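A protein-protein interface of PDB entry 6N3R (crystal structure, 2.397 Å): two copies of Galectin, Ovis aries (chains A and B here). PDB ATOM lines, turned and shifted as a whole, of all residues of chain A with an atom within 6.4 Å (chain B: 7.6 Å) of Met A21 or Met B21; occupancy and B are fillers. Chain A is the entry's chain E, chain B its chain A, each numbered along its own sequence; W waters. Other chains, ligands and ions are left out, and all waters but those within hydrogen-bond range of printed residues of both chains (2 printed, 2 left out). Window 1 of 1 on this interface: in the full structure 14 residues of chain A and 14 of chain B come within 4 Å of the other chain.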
ATOM      1  N   CYS A  19     -24.968 -27.755  28.825  1.00  0.00           N
ATOM      2  CA  CYS A  19     -25.162 -27.818  27.382  1.00  0.00           C
ATOM      3  C   CYS A  19     -24.532 -29.130  26.922  1.00  0.00           C
ATOM      4  O   CYS A  19     -23.352 -29.182  26.577  1.00  0.00           O
ATOM      5  CB  CYS A  19     -24.557 -26.620  26.675  1.00  0.00           C
ATOM      6  SG  CYS A  19     -24.913 -26.651  24.915  1.00  0.00           S
ATOM      7  N   TYR A  20     -25.337 -30.186  26.930  1.00  0.00           N
ATOM      8  CA  TYR A  20     -24.805 -31.535  26.822  1.00  0.00           C
ATOM      9  C   TYR A  20     -25.842 -32.391  26.125  1.00  0.00           C
ATOM     10  O   TYR A  20     -27.041 -32.260  26.390  1.00  0.00           O
ATOM     11  CB  TYR A  20     -24.462 -32.095  28.207  1.00  0.00           C
ATOM     12  CG  TYR A  20     -23.779 -33.443  28.227  1.00  0.00           C
ATOM     13  CD1 TYR A  20     -22.390 -33.541  28.344  1.00  0.00           C
ATOM     14  CD2 TYR A  20     -24.520 -34.625  28.144  1.00  0.00           C
ATOM     15  CE1 TYR A  20     -21.754 -34.789  28.384  1.00  0.00           C
ATOM     16  CE2 TYR A  20     -23.903 -35.872  28.169  1.00  0.00           C
ATOM     17  CZ  TYR A  20     -22.522 -35.951  28.304  1.00  0.00           C
ATOM     18  OH  TYR A  20     -21.916 -37.189  28.341  1.00  0.00           O
ATOM     19  N   MET A  21     -25.382 -33.246  25.220  1.00  0.00           N
ATOM     20  CA  MET A  21     -26.295 -34.029  24.415  1.00  0.00           C
ATOM     21  C   MET A  21     -25.910 -35.495  24.444  1.00  0.00           C
ATOM     22  O   MET A  21     -24.722 -35.848  24.390  1.00  0.00           O
ATOM     23  CB  MET A  21     -26.335 -33.553  22.973  1.00  0.00           C
ATOM     24  CG  MET A  21     -27.476 -34.209  22.168  1.00  0.00           C
ATOM     25  SD  MET A  21     -27.233 -34.020  20.394  1.00  0.00           S
ATOM     26  CE  MET A  21     -27.443 -32.248  20.228  1.00  0.00           C
ATOM     27  N   VAL A  22     -26.941 -36.334  24.536  1.00  0.00           N
ATOM     28  CA  VAL A  22     -26.853 -37.776  24.372  1.00  0.00           C
ATOM     29  C   VAL A  22     -27.687 -38.120  23.152  1.00  0.00           C
ATOM     30  O   VAL A  22     -28.869 -37.761  23.090  1.00  0.00           O
ATOM     31  CB  VAL A  22     -27.388 -38.530  25.603  1.00  0.00           C
ATOM     32  CG1 VAL A  22     -27.380 -40.033  25.348  1.00  0.00           C
ATOM     33  CG2 VAL A  22     -26.605 -38.161  26.860  1.00  0.00           C
ATOM     34  N   LYS A  23     -27.088 -38.808  22.184  1.00  0.00           N
ATOM     35  CA  LYS A  23     -27.833 -39.301  21.034  1.00  0.00           C
ATOM     36  C   LYS A  23     -27.738 -40.817  20.986  1.00  0.00           C
ATOM     37  O   LYS A  23     -26.632 -41.370  20.909  1.00  0.00           O
ATOM     38  CB  LYS A  23     -27.328 -38.697  19.723  1.00  0.00           C
ATOM     39  CG  LYS A  23     -28.048 -39.257  18.532  1.00  0.00           C
ATOM     40  CD  LYS A  23     -27.438 -38.791  17.246  1.00  0.00           C
ATOM     41  CE  LYS A  23     -27.750 -37.342  17.014  1.00  0.00           C
ATOM     42  NZ  LYS A  23     -27.271 -36.971  15.663  1.00  0.00           N
ATOM     43  N   GLN A  93     -32.810 -38.522  21.519  1.00  0.00           N
ATOM     44  CA  GLN A  93     -31.857 -37.522  21.969  1.00  0.00           C
ATOM     45  C   GLN A  93     -32.258 -37.010  23.334  1.00  0.00           C
ATOM     46  O   GLN A  93     -33.430 -36.694  23.560  1.00  0.00           O
ATOM     47  CB  GLN A  93     -31.769 -36.345  21.006  1.00  0.00           C
ATOM     48  CG  GLN A  93     -30.993 -36.617  19.748  1.00  0.00           C
ATOM     49  CD  GLN A  93     -31.136 -35.466  18.778  1.00  0.00           C
ATOM     50  OE1 GLN A  93     -32.208 -35.269  18.196  1.00  0.00           O
ATOM     51  NE2 GLN A  93     -30.082 -34.665  18.642  1.00  0.00           N
ATOM     52  N   PHE A  94     -31.276 -36.915  24.226  1.00  0.00           N
ATOM     53  CA  PHE A  94     -31.414 -36.194  25.481  1.00  0.00           C
ATOM     54  C   PHE A  94     -30.517 -34.961  25.428  1.00  0.00           C
ATOM     55  O   PHE A  94     -29.307 -35.062  25.187  1.00  0.00           O
ATOM     56  CB  PHE A  94     -31.079 -37.096  26.671  1.00  0.00           C
ATOM     57  CG  PHE A  94     -31.976 -38.310  26.769  1.00  0.00           C
ATOM     58  CD1 PHE A  94     -31.599 -39.517  26.188  1.00  0.00           C
ATOM     59  CD2 PHE A  94     -33.207 -38.231  27.408  1.00  0.00           C
ATOM     60  CE1 PHE A  94     -32.425 -40.639  26.249  1.00  0.00           C
ATOM     61  CE2 PHE A  94     -34.050 -39.344  27.474  1.00  0.00           C
ATOM     62  CZ  PHE A  94     -33.655 -40.552  26.890  1.00  0.00           C
ATOM     63  N   LEU A  95     -31.128 -33.801  25.617  1.00  0.00           N
ATOM     64  CA  LEU A  95     -30.435 -32.528  25.729  1.00  0.00           C
ATOM     65  C   LEU A  95     -30.472 -32.100  27.189  1.00  0.00           C
ATOM     66  O   LEU A  95     -31.554 -31.914  27.751  1.00  0.00           O
ATOM     67  CB  LEU A  95     -31.104 -31.479  24.841  1.00  0.00           C
ATOM     68  CG  LEU A  95     -30.341 -30.170  24.657  1.00  0.00           C
ATOM     69  CD1 LEU A  95     -28.899 -30.441  24.214  1.00  0.00           C
ATOM     70  CD2 LEU A  95     -31.081 -29.301  23.650  1.00  0.00           C
ATOM     71  N   VAL A  96     -29.304 -31.958  27.803  1.00  0.00           N
ATOM     72  CA  VAL A  96     -29.200 -31.529  29.193  1.00  0.00           C
ATOM     73  C   VAL A  96     -28.963 -30.026  29.209  1.00  0.00           C
ATOM     74  O   VAL A  96     -27.948 -29.545  28.689  1.00  0.00           O
ATOM     75  CB  VAL A  96     -28.077 -32.264  29.943  1.00  0.00           C
ATOM     76  CG1 VAL A  96     -28.044 -31.808  31.381  1.00  0.00           C
ATOM     77  CG2 VAL A  96     -28.265 -33.774  29.871  1.00  0.00           C
ATOM     78  N   ASP A 137     -23.854 -41.744  21.473  1.00  0.00           N
ATOM     79  CA  ASP A 137     -22.886 -40.668  21.335  1.00  0.00           C
ATOM     80  C   ASP A 137     -23.209 -39.558  22.319  1.00  0.00           C
ATOM     81  O   ASP A 137     -24.369 -39.370  22.703  1.00  0.00           O
ATOM     82  CB  ASP A 137     -22.859 -40.143  19.896  1.00  0.00           C
ATOM     83  CG  ASP A 137     -22.211 -41.118  18.960  1.00  0.00           C
ATOM     84  OD1 ASP A 137     -22.929 -41.800  18.205  1.00  0.00           O
ATOM     85  OD2 ASP A 137     -20.969 -41.247  19.026  1.00  0.00           O
ATOM     86  N   THR A 138     -22.167 -38.849  22.758  1.00  0.00           N
ATOM     87  CA  THR A 138     -22.350 -37.738  23.680  1.00  0.00           C
ATOM     88  C   THR A 138     -21.451 -36.582  23.284  1.00  0.00           C
ATOM     89  O   THR A 138     -20.313 -36.779  22.850  1.00  0.00           O
ATOM     90  CB  THR A 138     -22.058 -38.108  25.156  1.00  0.00           C
ATOM     91  OG1 THR A 138     -20.680 -38.470  25.305  1.00  0.00           O
ATOM     92  CG2 THR A 138     -22.955 -39.243  25.624  1.00  0.00           C
ATOM     93  N   LEU A 139     -21.971 -35.376  23.461  1.00  0.00           N
ATOM     94  CA  LEU A 139     -21.210 -34.161  23.268  1.00  0.00           C
ATOM     95  C   LEU A 139     -21.742 -33.138  24.264  1.00  0.00           C
ATOM     96  O   LEU A 139     -20.950 -32.382  24.818  1.00  0.00           O
ATOM     97  CB  LEU A 139     -21.324 -33.658  21.814  1.00  0.00           C
ATOM     98  CG  LEU A 139     -20.439 -32.492  21.359  1.00  0.00           C
ATOM     99  CD1 LEU A 139     -18.951 -32.896  21.408  1.00  0.00           C
ATOM    100  CD2 LEU A 139     -20.817 -32.039  19.946  1.00  0.00           C
ATOM    101  N   LEU B  16     -28.414 -29.083   9.914  1.00  0.00           N
ATOM    102  CA  LEU B  16     -28.866 -28.787  11.263  1.00  0.00           C
ATOM    103  C   LEU B  16     -30.207 -29.461  11.538  1.00  0.00           C
ATOM    104  O   LEU B  16     -30.934 -29.850  10.631  1.00  0.00           O
ATOM    105  CB  LEU B  16     -28.991 -27.283  11.475  1.00  0.00           C
ATOM    106  CG  LEU B  16     -27.758 -26.421  11.127  1.00  0.00           C
ATOM    107  CD1 LEU B  16     -27.970 -24.970  11.570  1.00  0.00           C
ATOM    108  CD2 LEU B  16     -26.457 -26.989  11.718  1.00  0.00           C
ATOM    109  N   THR B  17     -30.521 -29.606  12.820  1.00  0.00           N
ATOM    110  CA  THR B  17     -31.833 -30.029  13.272  1.00  0.00           C
ATOM    111  C   THR B  17     -32.261 -29.104  14.395  1.00  0.00           C
ATOM    112  O   THR B  17     -31.538 -28.175  14.779  1.00  0.00           O
ATOM    113  CB  THR B  17     -31.838 -31.473  13.790  1.00  0.00           C
ATOM    114  OG1 THR B  17     -31.048 -31.535  14.984  1.00  0.00           O
ATOM    115  CG2 THR B  17     -31.300 -32.457  12.760  1.00  0.00           C
ATOM    116  N   VAL B  18     -33.449 -29.382  14.944  1.00  0.00           N
ATOM    117  CA  VAL B  18     -33.930 -28.666  16.123  1.00  0.00           C
ATOM    118  C   VAL B  18     -33.246 -29.136  17.395  1.00  0.00           C
ATOM    119  O   VAL B  18     -33.559 -28.642  18.488  1.00  0.00           O
ATOM    120  CB  VAL B  18     -35.463 -28.816  16.230  1.00  0.00           C
ATOM    121  CG1 VAL B  18     -36.150 -28.204  15.003  1.00  0.00           C
ATOM    122  CG2 VAL B  18     -35.856 -30.298  16.406  1.00  0.00           C
ATOM    123  N   CYS B  19     -32.321 -30.084  17.294  1.00  0.00           N
ATOM    124  CA  CYS B  19     -31.561 -30.504  18.466  1.00  0.00           C
ATOM    125  C   CYS B  19     -30.170 -30.887  17.968  1.00  0.00           C
ATOM    126  O   CYS B  19     -29.891 -32.056  17.676  1.00  0.00           O
ATOM    127  CB  CYS B  19     -32.235 -31.650  19.203  1.00  0.00           C
ATOM    128  SG  CYS B  19     -31.365 -32.022  20.711  1.00  0.00           S
ATOM    129  N   TYR B  20     -29.304 -29.881  17.893  1.00  0.00           N
ATOM    130  CA  TYR B  20     -28.035 -29.991  17.192  1.00  0.00           C
ATOM    131  C   TYR B  20     -27.007 -29.143  17.927  1.00  0.00           C
ATOM    132  O   TYR B  20     -27.324 -28.045  18.390  1.00  0.00           O
ATOM    133  CB  TYR B  20     -28.184 -29.533  15.739  1.00  0.00           C
ATOM    134  CG  TYR B  20     -26.998 -29.822  14.851  1.00  0.00           C
ATOM    135  CD1 TYR B  20     -26.962 -30.957  14.055  1.00  0.00           C
ATOM    136  CD2 TYR B  20     -25.915 -28.958  14.810  1.00  0.00           C
ATOM    137  CE1 TYR B  20     -25.884 -31.221  13.234  1.00  0.00           C
ATOM    138  CE2 TYR B  20     -24.836 -29.211  13.996  1.00  0.00           C
ATOM    139  CZ  TYR B  20     -24.824 -30.335  13.200  1.00  0.00           C
ATOM    140  OH  TYR B  20     -23.740 -30.578  12.380  1.00  0.00           O
ATOM    141  N   MET B  21     -25.791 -29.664  18.051  1.00  0.00           N
ATOM    142  CA  MET B  21     -24.758 -29.010  18.837  1.00  0.00           C
ATOM    143  C   MET B  21     -23.460 -28.951  18.055  1.00  0.00           C
ATOM    144  O   MET B  21     -23.054 -29.934  17.426  1.00  0.00           O
ATOM    145  CB  MET B  21     -24.511 -29.716  20.159  1.00  0.00           C
ATOM    146  CG  MET B  21     -23.445 -28.991  20.983  1.00  0.00           C
ATOM    147  SD  MET B  21     -22.983 -29.887  22.469  1.00  0.00           S
ATOM    148  CE  MET B  21     -24.590 -30.081  23.246  1.00  0.00           C
ATOM    149  N   VAL B  22     -22.823 -27.786  18.094  1.00  0.00           N
ATOM    150  CA  VAL B  22     -21.471 -27.582  17.602  1.00  0.00           C
ATOM    151  C   VAL B  22     -20.610 -27.211  18.798  1.00  0.00           C
ATOM    152  O   VAL B  22     -20.989 -26.338  19.591  1.00  0.00           O
ATOM    153  CB  VAL B  22     -21.426 -26.480  16.530  1.00  0.00           C
ATOM    154  CG1 VAL B  22     -19.974 -26.166  16.137  1.00  0.00           C
ATOM    155  CG2 VAL B  22     -22.245 -26.906  15.323  1.00  0.00           C
ATOM    156  N   LYS B  23     -19.467 -27.875  18.939  1.00  0.00           N
ATOM    157  CA  LYS B  23     -18.522 -27.573  20.003  1.00  0.00           C
ATOM    158  C   LYS B  23     -17.163 -27.272  19.392  1.00  0.00           C
ATOM    159  O   LYS B  23     -16.543 -28.152  18.781  1.00  0.00           O
ATOM    160  CB  LYS B  23     -18.403 -28.720  21.002  1.00  0.00           C
ATOM    161  CG  LYS B  23     -17.423 -28.392  22.118  1.00  0.00           C
ATOM    162  CD  LYS B  23     -17.136 -29.587  22.993  1.00  0.00           C
ATOM    163  CE  LYS B  23     -18.361 -29.993  23.784  1.00  0.00           C
ATOM    164  NZ  LYS B  23     -18.015 -31.167  24.614  1.00  0.00           N
ATOM    165  N   ILE B  24     -16.705 -26.035  19.573  1.00  0.00           N
ATOM    166  CA  ILE B  24     -15.437 -25.546  19.052  1.00  0.00           C
ATOM    167  C   ILE B  24     -14.482 -25.354  20.220  1.00  0.00           C
ATOM    168  O   ILE B  24     -14.855 -24.775  21.249  1.00  0.00           O
ATOM    169  CB  ILE B  24     -15.627 -24.222  18.297  1.00  0.00           C
ATOM    170  CG1 ILE B  24     -16.464 -24.441  17.037  1.00  0.00           C
ATOM    171  CG2 ILE B  24     -14.275 -23.558  18.026  1.00  0.00           C
ATOM    172  CD1 ILE B  24     -17.169 -23.177  16.554  1.00  0.00           C
ATOM    173  N   PHE B  42     -22.746 -20.018  10.070  1.00  0.00           N
ATOM    174  CA  PHE B  42     -23.670 -21.071   9.676  1.00  0.00           C
ATOM    175  C   PHE B  42     -24.230 -20.596   8.341  1.00  0.00           C
ATOM    176  O   PHE B  42     -25.205 -19.840   8.287  1.00  0.00           O
ATOM    177  CB  PHE B  42     -24.753 -21.276  10.733  1.00  0.00           C
ATOM    178  CG  PHE B  42     -24.241 -21.830  12.026  1.00  0.00           C
ATOM    179  CD1 PHE B  42     -23.574 -21.017  12.925  1.00  0.00           C
ATOM    180  CD2 PHE B  42     -24.429 -23.167  12.352  1.00  0.00           C
ATOM    181  CE1 PHE B  42     -23.106 -21.518  14.113  1.00  0.00           C
ATOM    182  CE2 PHE B  42     -23.949 -23.676  13.548  1.00  0.00           C
ATOM    183  CZ  PHE B  42     -23.285 -22.851  14.423  1.00  0.00           C
ATOM    184  N   GLU B  91     -13.820 -23.000  25.213  1.00  0.00           N
ATOM    185  CA  GLU B  91     -14.755 -23.907  24.577  1.00  0.00           C
ATOM    186  C   GLU B  91     -15.981 -23.101  24.195  1.00  0.00           C
ATOM    187  O   GLU B  91     -16.619 -22.500  25.064  1.00  0.00           O
ATOM    188  CB  GLU B  91     -15.145 -25.044  25.509  1.00  0.00           C
ATOM    189  CG  GLU B  91     -16.224 -25.922  24.897  1.00  0.00           C
ATOM    190  CD  GLU B  91     -16.600 -27.102  25.766  1.00  0.00           C
ATOM    191  OE1 GLU B  91     -15.699 -27.736  26.374  1.00  0.00           O
ATOM    192  OE2 GLU B  91     -17.820 -27.378  25.853  1.00  0.00           O
ATOM    193  N   LEU B  92     -16.306 -23.090  22.907  1.00  0.00           N
ATOM    194  CA  LEU B  92     -17.431 -22.335  22.369  1.00  0.00           C
ATOM    195  C   LEU B  92     -18.460 -23.324  21.829  1.00  0.00           C
ATOM    196  O   LEU B  92     -18.133 -24.182  21.001  1.00  0.00           O
ATOM    197  CB  LEU B  92     -16.959 -21.366  21.281  1.00  0.00           C
ATOM    198  CG  LEU B  92     -18.003 -20.686  20.382  1.00  0.00           C
ATOM    199  CD1 LEU B  92     -18.884 -19.740  21.174  1.00  0.00           C
ATOM    200  CD2 LEU B  92     -17.329 -19.929  19.266  1.00  0.00           C
ATOM    201  N   GLN B  93     -19.692 -23.217  22.311  1.00  0.00           N
ATOM    202  CA  GLN B  93     -20.759 -24.129  21.938  1.00  0.00           C
ATOM    203  C   GLN B  93     -21.899 -23.363  21.283  1.00  0.00           C
ATOM    204  O   GLN B  93     -22.314 -22.311  21.771  1.00  0.00           O
ATOM    205  CB  GLN B  93     -21.299 -24.876  23.152  1.00  0.00           C
ATOM    206  CG  GLN B  93     -20.496 -26.072  23.569  1.00  0.00           C
ATOM    207  CD  GLN B  93     -21.040 -26.687  24.856  1.00  0.00           C
ATOM    208  OE1 GLN B  93     -21.017 -26.056  25.909  1.00  0.00           O
ATOM    209  NE2 GLN B  93     -21.554 -27.908  24.765  1.00  0.00           N
ATOM    210  N   PHE B  94     -22.408 -23.908  20.187  1.00  0.00           N
ATOM    211  CA  PHE B  94     -23.652 -23.459  19.589  1.00  0.00           C
ATOM    212  C   PHE B  94     -24.664 -24.577  19.717  1.00  0.00           C
ATOM    213  O   PHE B  94     -24.392 -25.716  19.322  1.00  0.00           O
ATOM    214  CB  PHE B  94     -23.460 -23.082  18.120  1.00  0.00           C
ATOM    215  CG  PHE B  94     -22.557 -21.916  17.926  1.00  0.00           C
ATOM    216  CD1 PHE B  94     -21.201 -22.107  17.694  1.00  0.00           C
ATOM    217  CD2 PHE B  94     -23.051 -20.624  18.011  1.00  0.00           C
ATOM    218  CE1 PHE B  94     -20.347 -21.009  17.523  1.00  0.00           C
ATOM    219  CE2 PHE B  94     -22.206 -19.531  17.850  1.00  0.00           C
ATOM    220  CZ  PHE B  94     -20.859 -19.721  17.606  1.00  0.00           C
ATOM    221  N   LEU B  95     -25.819 -24.256  20.272  1.00  0.00           N
ATOM    222  CA  LEU B  95     -26.927 -25.192  20.381  1.00  0.00           C
ATOM    223  C   LEU B  95     -28.024 -24.729  19.429  1.00  0.00           C
ATOM    224  O   LEU B  95     -28.515 -23.599  19.538  1.00  0.00           O
ATOM    225  CB  LEU B  95     -27.417 -25.247  21.826  1.00  0.00           C
ATOM    226  CG  LEU B  95     -28.525 -26.230  22.120  1.00  0.00           C
ATOM    227  CD1 LEU B  95     -28.141 -27.642  21.614  1.00  0.00           C
ATOM    228  CD2 LEU B  95     -28.817 -26.194  23.622  1.00  0.00           C
ATOM    229  N   VAL B  96     -28.374 -25.572  18.468  1.00  0.00           N
ATOM    230  CA  VAL B  96     -29.420 -25.247  17.511  1.00  0.00           C
ATOM    231  C   VAL B  96     -30.733 -25.842  18.024  1.00  0.00           C
ATOM    232  O   VAL B  96     -30.894 -27.064  18.077  1.00  0.00           O
ATOM    233  CB  VAL B  96     -29.083 -25.770  16.109  1.00  0.00           C
ATOM    234  CG1 VAL B  96     -30.062 -25.202  15.098  1.00  0.00           C
ATOM    235  CG2 VAL B  96     -27.665 -25.425  15.743  1.00  0.00           C
ATOM    236  N   LEU B  97     -31.662 -24.979  18.415  1.00  0.00           N
ATOM    237  CA  LEU B  97     -33.012 -25.360  18.814  1.00  0.00           C
ATOM    238  C   LEU B  97     -33.992 -24.897  17.745  1.00  0.00           C
ATOM    239  O   LEU B  97     -33.631 -24.157  16.827  1.00  0.00           O
ATOM    240  CB  LEU B  97     -33.365 -24.760  20.186  1.00  0.00           C
ATOM    241  CG  LEU B  97     -32.389 -25.151  21.308  1.00  0.00           C
ATOM    242  CD1 LEU B  97     -32.799 -24.584  22.663  1.00  0.00           C
ATOM    243  CD2 LEU B  97     -32.242 -26.667  21.372  1.00  0.00           C
ATOM    244  N   PHE B 104     -22.762 -20.767  24.165  1.00  0.00           N
ATOM    245  CA  PHE B 104     -22.114 -20.994  25.454  1.00  0.00           C
ATOM    246  C   PHE B 104     -20.612 -20.888  25.269  1.00  0.00           C
ATOM    247  O   PHE B 104     -20.072 -21.318  24.246  1.00  0.00           O
ATOM    248  CB  PHE B 104     -22.442 -22.377  26.051  1.00  0.00           C
ATOM    249  CG  PHE B 104     -23.903 -22.614  26.291  1.00  0.00           C
ATOM    250  CD1 PHE B 104     -24.763 -22.893  25.229  1.00  0.00           C
ATOM    251  CD2 PHE B 104     -24.414 -22.597  27.588  1.00  0.00           C
ATOM    252  CE1 PHE B 104     -26.112 -23.128  25.450  1.00  0.00           C
ATOM    253  CE2 PHE B 104     -25.772 -22.833  27.827  1.00  0.00           C
ATOM    254  CZ  PHE B 104     -26.622 -23.094  26.757  1.00  0.00           C
ATOM    255  N   ASP B 137     -16.455 -30.234  16.818  1.00  0.00           N
ATOM    256  CA  ASP B 137     -17.305 -31.402  16.915  1.00  0.00           C
ATOM    257  C   ASP B 137     -18.761 -30.998  16.780  1.00  0.00           C
ATOM    258  O   ASP B 137     -19.166 -29.922  17.233  1.00  0.00           O
ATOM    259  CB  ASP B 137     -17.088 -32.129  18.235  1.00  0.00           C
ATOM    260  CG  ASP B 137     -15.760 -32.801  18.294  1.00  0.00           C
ATOM    261  OD1 ASP B 137     -15.580 -33.801  17.576  1.00  0.00           O
ATOM    262  OD2 ASP B 137     -14.888 -32.327  19.034  1.00  0.00           O
ATOM    263  N   THR B 138     -19.540 -31.865  16.137  1.00  0.00           N
ATOM    264  CA  THR B 138     -20.965 -31.652  15.969  1.00  0.00           C
ATOM    265  C   THR B 138     -21.701 -32.942  16.287  1.00  0.00           C
ATOM    266  O   THR B 138     -21.219 -34.041  15.995  1.00  0.00           O
ATOM    267  CB  THR B 138     -21.334 -31.196  14.546  1.00  0.00           C
ATOM    268  OG1 THR B 138     -21.134 -32.273  13.626  1.00  0.00           O
ATOM    269  CG2 THR B 138     -20.513 -29.962  14.116  1.00  0.00           C
ATOM    270  N   LEU B 139     -22.865 -32.784  16.884  1.00  0.00           N
ATOM    271  CA  LEU B 139     -23.784 -33.861  17.182  1.00  0.00           C
ATOM    272  C   LEU B 139     -25.203 -33.278  17.163  1.00  0.00           C
ATOM    273  O   LEU B 139     -26.114 -33.942  16.653  1.00  0.00           O
ATOM    274  CB  LEU B 139     -23.468 -34.506  18.539  1.00  0.00           C
ATOM    275  CG  LEU B 139     -24.323 -35.717  18.890  1.00  0.00           C
ATOM    276  CD1 LEU B 139     -23.973 -36.901  17.974  1.00  0.00           C
ATOM    277  CD2 LEU B 139     -24.128 -36.089  20.360  1.00  0.00           C
HETATM  278  O   HOH W   1     -21.102 -27.508  28.339  1.00  0.00           O
HETATM  279  O   HOH W   2     -28.448 -33.515  15.869  1.00  0.00           O
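O of Cys B19 sits at hydrogen-bond distance from NE2 of Gln A93, at 2.8 Å. The side-chain amino group of Lys B23 lies within hydrogen-bond range of the backbone carbonyl oxygen of Leu A139, at 3.2 Å. The side-chain amide nitrogen (NE2) of Gln B93 lies within hydrogen-bond range of the backbone carbonyl oxygen (O) of Cys A19, at 2.9 Å. The backbone carbonyl oxygen of Leu B139 sits at hydrogen-bond distance from the side-chain amino group of Lys A23.
OG1 of Thr B17 sits at hydrogen-bond distance from O of Cys B19. The backbone carbonyl oxygen (O) of Tyr B20 lies within hydrogen-bond range of the backbone NH (N) of Val B96, at 2.7 Å. The backbone NH (N) of Leu B139 sits at hydrogen-bond distance from the backbone carbonyl oxygen (O) of Met B21 (2.9 Å). The backbone NH (N) of Gln B93 lies within hydrogen-bond range of the backbone carbonyl oxygen (O) of Phe B104 (2.7 Å). The backbone NH (N) of Cys A19 lies within hydrogen-bond range of the backbone carbonyl oxygen (O) of Val A96, at 3.5 Å. The backbone NH of Lys A23 is in hydrogen-bond range of the backbone carbonyl oxygen of Asp A137.
Cys A19 touches Met B21 (O to CE, 3.7 Å). Tyr A20 touches Met B21 (N to CE, 3.8 Å). Met B21 touches Met A21. Leu B95 touches Leu A95 (CD2 to CD2, 3.8 Å). Leu A95 touches Leu B97 (CD2 to CD2, 3.7 Å). CB of Asp A137 touches CD1 of Leu B139, 3.9 Å away. Leu A139 touches Met B21 (CG to SD, 3.8 Å). CD1 of Leu A139 touches CB of Asp B137 (3.8 Å). C of Thr B138 touches CD2 of Leu A139, at 3.9 Å. CD2 of Leu A139 touches N of Leu B139 (3.8 Å).
Of chain B, only Cys B19, Tyr B20, Met B21 and Leu B139 come within 4 Å of Met A21. Met B21 touches four residues of chain A. Of the printed residues of chain A, Leu B139 touches Met A21, Lys A23, Asp A137, Thr A138 and Leu A139. Of the printed residues of chain A, Leu B97 touches Leu A95. Printed residues of chain A within 4 Å of Lys B23: Leu A139 (3.2 Å). Of the printed residues of chain B, Lys A23 touches Leu B139 (3.4 Å). Of the printed residues of chain A, Thr B138 touches Leu A139. Val B96 touches none of the printed residues of chain A. The nearest residue of chain B that does not touch Met A21 is Leu B95 (4.9 Å). The nearest residue of chain A that does not touch Met B21 is Leu A95 (4.4 Å).
Printed residues of chain B that touch a printed residue of chain A: Cys B19, Tyr B20, Met B21, Lys B23, Gln B93, Leu B95, Leu B97, Phe B104, Asp B137, Thr B138 and Leu B139. Hydrophobic or aromatic side chains of chain B that line the printed part of chain A: Met B21, Leu B95, Leu B97, Phe B104 and Leu B139. Along chain B the printed residues that touch a printed residue of chain A span positions 19 to 139. Printed residues of chain A that touch a printed residue of chain B: Cys A19, Tyr A20, Met A21, Lys A23, Gln A93, Leu A95, Asp A137, Thr A138 and Leu A139. Among the printed residues, 19 pairs touch across the chains. Among the printed residues, no Asp or Glu carboxylate lies within 4 Å of a Lys or Arg side-chain nitrogen of the other chain.
Tyr A20 touches Met B21, and with the chains exchanged Met A21 touches Tyr B20. Leu B95 touches its own counterpart, Leu A95. Asp A137 touches Leu B139, and with the chains exchanged Leu A139 touches Asp B137. Leu B139 touches its own counterpart, Leu A139.
Water W2 lies within hydrogen-bond range of O of Leu B139, O of Cys B19, OG1 of Thr B17 and NE2 of Gln A93. Water W1 lies within hydrogen-bond range of OE1 of Gln B93 (2.8 Å) and O of Cys A19 (3.3 Å).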
